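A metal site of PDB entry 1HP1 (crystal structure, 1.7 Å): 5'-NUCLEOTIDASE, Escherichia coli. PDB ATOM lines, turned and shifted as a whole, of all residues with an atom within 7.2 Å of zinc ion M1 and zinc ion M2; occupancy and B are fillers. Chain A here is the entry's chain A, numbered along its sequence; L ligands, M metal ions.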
ATOM      1  N   ASN A  15     -15.603  36.842  26.524  1.00  0.00           N
ATOM      2  CA  ASN A  15     -15.931  35.416  26.634  1.00  0.00           C
ATOM      3  C   ASN A  15     -16.191  35.057  28.090  1.00  0.00           C
ATOM      4  O   ASN A  15     -15.780  35.773  28.998  1.00  0.00           O
ATOM      5  CB  ASN A  15     -14.758  34.559  26.124  1.00  0.00           C
ATOM      6  CG  ASN A  15     -13.456  34.861  26.859  1.00  0.00           C
ATOM      7  OD1 ASN A  15     -12.769  35.833  26.545  1.00  0.00           O
ATOM      8  ND2 ASN A  15     -13.133  34.051  27.870  1.00  0.00           N
ATOM      9  N   ASP A  16     -16.876  33.935  28.295  1.00  0.00           N
ATOM     10  CA  ASP A  16     -17.107  33.405  29.633  1.00  0.00           C
ATOM     11  C   ASP A  16     -17.699  34.439  30.571  1.00  0.00           C
ATOM     12  O   ASP A  16     -17.304  34.601  31.726  1.00  0.00           O
ATOM     13  CB  ASP A  16     -15.795  32.815  30.161  1.00  0.00           C
ATOM     14  CG  ASP A  16     -15.343  31.652  29.301  1.00  0.00           C
ATOM     15  OD1 ASP A  16     -14.684  31.855  28.289  1.00  0.00           O
ATOM     16  OD2 ASP A  16     -15.716  30.515  29.601  1.00  0.00           O
ATOM     17  N   HIS A  17     -18.713  35.105  30.046  1.00  0.00           N
ATOM     18  CA  HIS A  17     -19.467  36.126  30.753  1.00  0.00           C
ATOM     19  C   HIS A  17     -20.087  35.519  32.030  1.00  0.00           C
ATOM     20  O   HIS A  17     -20.123  36.158  33.075  1.00  0.00           O
ATOM     21  CB  HIS A  17     -20.524  36.622  29.780  1.00  0.00           C
ATOM     22  CG  HIS A  17     -21.501  37.568  30.381  1.00  0.00           C
ATOM     23  ND1 HIS A  17     -21.198  38.880  30.680  1.00  0.00           N
ATOM     24  CD2 HIS A  17     -22.785  37.371  30.780  1.00  0.00           C
ATOM     25  CE1 HIS A  17     -22.247  39.453  31.240  1.00  0.00           C
ATOM     26  NE2 HIS A  17     -23.231  38.563  31.306  1.00  0.00           N
ATOM     27  N   HIS A  18     -20.600  34.300  31.927  1.00  0.00           N
ATOM     28  CA  HIS A  18     -21.142  33.589  33.082  1.00  0.00           C
ATOM     29  C   HIS A  18     -22.066  34.337  34.003  1.00  0.00           C
ATOM     30  O   HIS A  18     -21.849  34.394  35.224  1.00  0.00           O
ATOM     31  CB  HIS A  18     -19.987  32.985  33.883  1.00  0.00           C
ATOM     32  CG  HIS A  18     -19.375  31.806  33.215  1.00  0.00           C
ATOM     33  ND1 HIS A  18     -20.115  30.683  32.888  1.00  0.00           N
ATOM     34  CD2 HIS A  18     -18.118  31.571  32.795  1.00  0.00           C
ATOM     35  CE1 HIS A  18     -19.324  29.802  32.298  1.00  0.00           C
ATOM     36  NE2 HIS A  18     -18.113  30.316  32.228  1.00  0.00           N
ATOM     37  N   GLY A  57     -16.818  34.575  22.903  1.00  0.00           N
ATOM     38  CA  GLY A  57     -16.337  33.207  22.932  1.00  0.00           C
ATOM     39  C   GLY A  57     -17.297  32.266  23.677  1.00  0.00           C
ATOM     40  O   GLY A  57     -16.959  31.113  23.930  1.00  0.00           O
ATOM     41  N   GLY A  58     -18.466  32.761  24.053  1.00  0.00           N
ATOM     42  CA  GLY A  58     -19.442  31.877  24.691  1.00  0.00           C
ATOM     43  C   GLY A  58     -19.409  31.737  26.191  1.00  0.00           C
ATOM     44  O   GLY A  58     -18.625  32.387  26.872  1.00  0.00           O
ATOM     45  N   ASP A  59     -20.251  30.847  26.710  1.00  0.00           N
ATOM     46  CA  ASP A  59     -20.414  30.636  28.151  1.00  0.00           C
ATOM     47  C   ASP A  59     -21.027  31.885  28.761  1.00  0.00           C
ATOM     48  O   ASP A  59     -20.466  32.526  29.660  1.00  0.00           O
ATOM     49  CB  ASP A  59     -19.103  30.244  28.862  1.00  0.00           C
ATOM     50  CG  ASP A  59     -18.950  28.746  28.983  1.00  0.00           C
ATOM     51  OD1 ASP A  59     -19.730  27.973  28.387  1.00  0.00           O
ATOM     52  OD2 ASP A  59     -18.016  28.308  29.682  1.00  0.00           O
ATOM     53  N   ILE A  60     -22.211  32.230  28.269  1.00  0.00           N
ATOM     54  CA  ILE A  60     -22.952  33.372  28.783  1.00  0.00           C
ATOM     55  C   ILE A  60     -23.674  32.867  30.014  1.00  0.00           C
ATOM     56  O   ILE A  60     -23.865  33.593  30.990  1.00  0.00           O
ATOM     57  CB  ILE A  60     -24.002  33.838  27.747  1.00  0.00           C
ATOM     58  CG1 ILE A  60     -23.302  34.141  26.424  1.00  0.00           C
ATOM     59  CG2 ILE A  60     -24.769  35.079  28.277  1.00  0.00           C
ATOM     60  CD1 ILE A  60     -22.084  35.066  26.572  1.00  0.00           C
ATOM     61  N   ASN A  61     -24.096  31.598  29.952  1.00  0.00           N
ATOM     62  CA  ASN A  61     -24.811  30.984  31.061  1.00  0.00           C
ATOM     63  C   ASN A  61     -23.956  30.559  32.233  1.00  0.00           C
ATOM     64  O   ASN A  61     -22.799  30.139  32.073  1.00  0.00           O
ATOM     65  CB  ASN A  61     -25.483  29.669  30.616  1.00  0.00           C
ATOM     66  CG  ASN A  61     -26.700  29.891  29.772  1.00  0.00           C
ATOM     67  OD1 ASN A  61     -27.807  29.997  30.287  1.00  0.00           O
ATOM     68  ND2 ASN A  61     -26.506  29.963  28.443  1.00  0.00           N
ATOM     69  N   THR A  62     -24.617  30.645  33.388  1.00  0.00           N
ATOM     70  CA  THR A  62     -24.188  30.096  34.654  1.00  0.00           C
ATOM     71  C   THR A  62     -23.083  30.707  35.446  1.00  0.00           C
ATOM     72  O   THR A  62     -21.941  30.698  35.010  1.00  0.00           O
ATOM     73  CB  THR A  62     -23.897  28.618  34.443  1.00  0.00           C
ATOM     74  OG1 THR A  62     -24.954  28.064  33.636  1.00  0.00           O
ATOM     75  CG2 THR A  62     -23.815  27.874  35.802  1.00  0.00           C
ATOM     76  N   GLY A  90     -20.884  27.915  24.027  1.00  0.00           N
ATOM     77  CA  GLY A  90     -19.993  27.353  25.032  1.00  0.00           C
ATOM     78  C   GLY A  90     -20.549  26.120  25.688  1.00  0.00           C
ATOM     79  O   GLY A  90     -21.741  25.813  25.532  1.00  0.00           O
ATOM     80  N   ASN A  91     -19.719  25.392  26.446  1.00  0.00           N
ATOM     81  CA  ASN A  91     -20.270  24.196  27.103  1.00  0.00           C
ATOM     82  C   ASN A  91     -21.356  24.520  28.110  1.00  0.00           C
ATOM     83  O   ASN A  91     -22.273  23.716  28.299  1.00  0.00           O
ATOM     84  CB  ASN A  91     -19.155  23.374  27.779  1.00  0.00           C
ATOM     85  CG  ASN A  91     -18.378  24.155  28.816  1.00  0.00           C
ATOM     86  OD1 ASN A  91     -17.909  25.238  28.551  1.00  0.00           O
ATOM     87  ND2 ASN A  91     -18.215  23.586  30.013  1.00  0.00           N
ATOM     88  N   HIS A  92     -21.289  25.685  28.773  1.00  0.00           N
ATOM     89  CA  HIS A  92     -22.345  25.982  29.734  1.00  0.00           C
ATOM     90  C   HIS A  92     -23.674  26.367  29.108  1.00  0.00           C
ATOM     91  O   HIS A  92     -24.674  26.484  29.786  1.00  0.00           O
ATOM     92  CB  HIS A  92     -21.839  27.039  30.730  1.00  0.00           C
ATOM     93  CG  HIS A  92     -20.877  26.483  31.735  1.00  0.00           C
ATOM     94  ND1 HIS A  92     -21.282  25.865  32.905  1.00  0.00           N
ATOM     95  CD2 HIS A  92     -19.530  26.401  31.713  1.00  0.00           C
ATOM     96  CE1 HIS A  92     -20.217  25.421  33.549  1.00  0.00           C
ATOM     97  NE2 HIS A  92     -19.147  25.734  32.858  1.00  0.00           N
ATOM     98  N   THR A 147     -15.969  23.221  22.468  1.00  0.00           N
ATOM     99  CA  THR A 147     -15.149  22.127  22.945  1.00  0.00           C
ATOM    100  C   THR A 147     -15.874  20.783  22.945  1.00  0.00           C
ATOM    101  O   THR A 147     -17.046  20.709  23.327  1.00  0.00           O
ATOM    102  CB  THR A 147     -14.603  22.384  24.369  1.00  0.00           C
ATOM    103  OG1 THR A 147     -13.892  21.215  24.779  1.00  0.00           O
ATOM    104  CG2 THR A 147     -15.714  22.689  25.377  1.00  0.00           C
ATOM    105  N   THR A 150     -17.603  19.017  26.084  1.00  0.00           N
ATOM    106  CA  THR A 150     -18.899  19.455  26.640  1.00  0.00           C
ATOM    107  C   THR A 150     -19.780  18.370  27.256  1.00  0.00           C
ATOM    108  O   THR A 150     -20.252  18.514  28.386  1.00  0.00           O
ATOM    109  CB  THR A 150     -19.716  20.230  25.560  1.00  0.00           C
ATOM    110  OG1 THR A 150     -18.986  21.420  25.199  1.00  0.00           O
ATOM    111  CG2 THR A 150     -21.098  20.669  26.089  1.00  0.00           C
ATOM    112  N   ILE A 153     -17.704  15.947  30.375  1.00  0.00           N
ATOM    113  CA  ILE A 153     -17.374  16.262  31.734  1.00  0.00           C
ATOM    114  C   ILE A 153     -18.475  16.283  32.753  1.00  0.00           C
ATOM    115  O   ILE A 153     -19.650  16.510  32.470  1.00  0.00           O
ATOM    116  CB  ILE A 153     -16.567  17.544  31.801  1.00  0.00           C
ATOM    117  CG1 ILE A 153     -17.349  18.674  31.160  1.00  0.00           C
ATOM    118  CG2 ILE A 153     -15.230  17.369  31.038  1.00  0.00           C
ATOM    119  CD1 ILE A 153     -16.448  19.924  30.882  1.00  0.00           C
ATOM    120  N   HIS A 192     -14.835  28.027  21.738  1.00  0.00           N
ATOM    121  CA  HIS A 192     -14.964  27.845  23.166  1.00  0.00           C
ATOM    122  C   HIS A 192     -14.190  26.580  23.412  1.00  0.00           C
ATOM    123  O   HIS A 192     -14.757  25.513  23.687  1.00  0.00           O
ATOM    124  CB  HIS A 192     -16.410  27.646  23.545  1.00  0.00           C
ATOM    125  CG  HIS A 192     -16.610  27.805  24.997  1.00  0.00           C
ATOM    126  ND1 HIS A 192     -16.660  29.037  25.591  1.00  0.00           N
ATOM    127  CD2 HIS A 192     -16.553  26.891  26.003  1.00  0.00           C
ATOM    128  CE1 HIS A 192     -16.620  28.900  26.905  1.00  0.00           C
ATOM    129  NE2 HIS A 192     -16.553  27.614  27.175  1.00  0.00           N
ATOM    130  N   MET A 193     -12.874  26.715  23.350  1.00  0.00           N
ATOM    131  CA  MET A 193     -12.013  25.529  23.372  1.00  0.00           C
ATOM    132  C   MET A 193     -10.871  25.575  24.377  1.00  0.00           C
ATOM    133  O   MET A 193     -10.375  24.525  24.793  1.00  0.00           O
ATOM    134  CB  MET A 193     -11.467  25.315  21.952  1.00  0.00           C
ATOM    135  CG  MET A 193     -12.559  24.836  20.976  1.00  0.00           C
ATOM    136  SD  MET A 193     -12.020  24.907  19.220  1.00  0.00           S
ATOM    137  CE  MET A 193     -10.477  23.986  19.306  1.00  0.00           C
ATOM    138  N   GLY A 226     -12.100  31.162  24.457  1.00  0.00           N
ATOM    139  CA  GLY A 226     -12.764  31.185  25.759  1.00  0.00           C
ATOM    140  C   GLY A 226     -12.510  29.869  26.450  1.00  0.00           C
ATOM    141  O   GLY A 226     -11.541  29.179  26.136  1.00  0.00           O
ATOM    142  N   HIS A 227     -13.405  29.541  27.384  1.00  0.00           N
ATOM    143  CA  HIS A 227     -13.387  28.281  28.132  1.00  0.00           C
ATOM    144  C   HIS A 227     -12.338  28.156  29.219  1.00  0.00           C
ATOM    145  O   HIS A 227     -12.696  27.920  30.380  1.00  0.00           O
ATOM    146  CB  HIS A 227     -13.300  27.074  27.163  1.00  0.00           C
ATOM    147  CG  HIS A 227     -13.541  25.749  27.841  1.00  0.00           C
ATOM    148  ND1 HIS A 227     -14.606  25.515  28.677  1.00  0.00           N
ATOM    149  CD2 HIS A 227     -12.848  24.592  27.797  1.00  0.00           C
ATOM    150  CE1 HIS A 227     -14.556  24.278  29.129  1.00  0.00           C
ATOM    151  NE2 HIS A 227     -13.493  23.695  28.612  1.00  0.00           N
ATOM    152  N   SER A 228     -11.059  28.321  28.856  1.00  0.00           N
ATOM    153  CA  SER A 228     -10.002  28.215  29.847  1.00  0.00           C
ATOM    154  C   SER A 228     -10.023  29.398  30.839  1.00  0.00           C
ATOM    155  O   SER A 228      -9.504  29.284  31.957  1.00  0.00           O
ATOM    156  CB  SER A 228      -8.628  28.065  29.171  1.00  0.00           C
ATOM    157  OG  SER A 228      -8.349  29.120  28.263  1.00  0.00           O
ATOM    158  N   GLN A 229     -10.668  30.483  30.425  1.00  0.00           N
ATOM    159  CA  GLN A 229     -10.847  31.698  31.207  1.00  0.00           C
ATOM    160  C   GLN A 229      -9.552  32.350  31.619  1.00  0.00           C
ATOM    161  O   GLN A 229      -9.189  32.394  32.813  1.00  0.00           O
ATOM    162  CB  GLN A 229     -11.759  31.420  32.416  1.00  0.00           C
ATOM    163  CG  GLN A 229     -13.156  31.062  31.901  1.00  0.00           C
ATOM    164  CD  GLN A 229     -14.228  30.894  32.974  1.00  0.00           C
ATOM    165  OE1 GLN A 229     -15.210  30.186  32.757  1.00  0.00           O
ATOM    166  NE2 GLN A 229     -14.090  31.576  34.099  1.00  0.00           N
ATOM    167  N   HIS A 264     -10.319  36.716  29.328  1.00  0.00           N
ATOM    168  CA  HIS A 264     -10.511  36.229  30.678  1.00  0.00           C
ATOM    169  C   HIS A 264     -11.924  35.751  30.976  1.00  0.00           C
ATOM    170  O   HIS A 264     -12.272  34.657  30.571  1.00  0.00           O
ATOM    171  CB  HIS A 264     -10.015  37.261  31.704  1.00  0.00           C
ATOM    172  CG  HIS A 264      -9.691  36.639  33.027  1.00  0.00           C
ATOM    173  ND1 HIS A 264      -9.040  37.317  34.048  1.00  0.00           N
ATOM    174  CD2 HIS A 264      -9.967  35.412  33.497  1.00  0.00           C
ATOM    175  CE1 HIS A 264      -8.939  36.517  35.094  1.00  0.00           C
ATOM    176  NE2 HIS A 264      -9.506  35.354  34.802  1.00  0.00           N
ATOM    177  N   GLU A 265     -12.745  36.547  31.633  1.00  0.00           N
ATOM    178  CA  GLU A 265     -14.090  36.088  31.992  1.00  0.00           C
ATOM    179  C   GLU A 265     -14.897  37.245  32.568  1.00  0.00           C
ATOM    180  O   GLU A 265     -14.342  38.299  32.845  1.00  0.00           O
ATOM    181  CB  GLU A 265     -13.950  35.043  33.110  1.00  0.00           C
ATOM    182  CG  GLU A 265     -13.357  35.708  34.377  1.00  0.00           C
ATOM    183  CD  GLU A 265     -12.817  34.756  35.407  1.00  0.00           C
ATOM    184  OE1 GLU A 265     -12.741  33.521  35.147  1.00  0.00           O
ATOM    185  OE2 GLU A 265     -12.445  35.257  36.488  1.00  0.00           O
ATOM    186  N   TRP A 266     -16.209  37.020  32.700  1.00  0.00           N
ATOM    187  CA  TRP A 266     -17.119  37.902  33.424  1.00  0.00           C
ATOM    188  C   TRP A 266     -17.229  39.339  32.984  1.00  0.00           C
ATOM    189  O   TRP A 266     -17.571  40.197  33.808  1.00  0.00           O
ATOM    190  CB  TRP A 266     -16.736  37.929  34.927  1.00  0.00           C
ATOM    191  CG  TRP A 266     -16.655  36.574  35.619  1.00  0.00           C
ATOM    192  CD1 TRP A 266     -16.964  35.342  35.089  1.00  0.00           C
ATOM    193  CD2 TRP A 266     -16.291  36.343  36.976  1.00  0.00           C
ATOM    194  NE1 TRP A 266     -16.820  34.360  36.060  1.00  0.00           N
ATOM    195  CE2 TRP A 266     -16.413  34.959  37.220  1.00  0.00           C
ATOM    196  CE3 TRP A 266     -15.874  37.183  38.010  1.00  0.00           C
ATOM    197  CZ2 TRP A 266     -16.131  34.383  38.461  1.00  0.00           C
ATOM    198  CZ3 TRP A 266     -15.599  36.610  39.259  1.00  0.00           C
ATOM    199  CH2 TRP A 266     -15.736  35.223  39.464  1.00  0.00           C
ATOM    200  N   THR A 484     -15.106  22.907  36.919  1.00  0.00           N
ATOM    201  CA  THR A 484     -16.400  22.872  36.222  1.00  0.00           C
ATOM    202  C   THR A 484     -17.049  24.217  35.973  1.00  0.00           C
ATOM    203  O   THR A 484     -17.979  24.293  35.139  1.00  0.00           O
ATOM    204  CB  THR A 484     -17.414  22.050  37.007  1.00  0.00           C
ATOM    205  OG1 THR A 484     -17.840  22.800  38.164  1.00  0.00           O
ATOM    206  CG2 THR A 484     -16.769  20.731  37.484  1.00  0.00           C
ATOM    207  N   GLY A 485     -16.622  25.245  36.675  1.00  0.00           N
ATOM    208  CA  GLY A 485     -17.239  26.564  36.518  1.00  0.00           C
ATOM    209  C   GLY A 485     -18.521  26.722  37.318  1.00  0.00           C
ATOM    210  O   GLY A 485     -19.151  27.794  37.315  1.00  0.00           O
HETATM  211  C1  LIG L   1     -16.108  26.104  32.122  1.00  0.00           C
HETATM  212  O1  LIG L   1     -15.562  27.069  31.536  1.00  0.00           O
HETATM  213  O2  LIG L   1     -16.141  25.964  33.378  1.00  0.00           O
HETATM  214  O3  LIG L   1     -16.670  25.261  31.379  1.00  0.00           O
HETATM  215 ZN    ZN M   1     -16.600  29.413  31.116  1.00  0.00          ZN
HETATM  216 ZN    ZN M   2     -16.540  26.739  29.052  1.00  0.00          ZN
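A ring nitrogen (NE2) of His 192 binds zinc ion M2, at 2.1 Å. OD1 of Asn 91 is bound to zinc ion M2 (2.1 Å). Zinc ion M2 is bound by OD2 of Asp 59 (2.2 Å). ND1 of His 227 is bound to zinc ion M2. Slightly farther from zinc ion M2 lies an oxygen (O1) of the ligand (2.7 Å). Slightly farther from zinc ion M2 lies O3 of the ligand (2.8 Å).
Within 4 Å of zinc ion M1: Asp 16, His 18, Asp 59 and Gln 229.
Of the 27 residues printed, 5 come within 4 Å of zinc ion M2.
Zinc ion M1 is bound by OD2 of Asp 16. NE2 of His 18 binds zinc ion M1 (2.1 Å). OE1 of Gln 229 is bound to zinc ion M1 (2.3 Å). OD2 of Asp 59 is bound to zinc ion M1 (2.3 Å). An oxygen (O1) of the ligand binds zinc ion M1 (2.6 Å).
The side-chain carboxylate (OD1) of Asp 59 sits at hydrogen-bond distance from the backbone NH (N) of His 92, at 2.8 Å. O of Gly 58 sits at hydrogen-bond distance from N of Asp 16 (2.7 Å). A ring nitrogen (ND1) of His 192 sits at hydrogen-bond distance from the backbone carbonyl oxygen (O) of Gly 57 (2.7 Å). The side-chain amide nitrogen (NE2) of Gln 229 sits at hydrogen-bond distance from the side-chain carboxylate (OE1) of Glu 265, at 2.6 Å. N of His 18 lies close to O of Ile 60 (3.5 Å). The side-chain amide nitrogen (ND2) of Asn 15 lies within hydrogen-bond range of the side-chain carboxylate (OD1) of Asp 16 (2.7 Å). The backbone NH of His 227 sits at hydrogen-bond distance from the side-chain carboxylate of Asp 16 (2.8 Å). N of Thr 147 lies within hydrogen-bond range of O of His 192.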
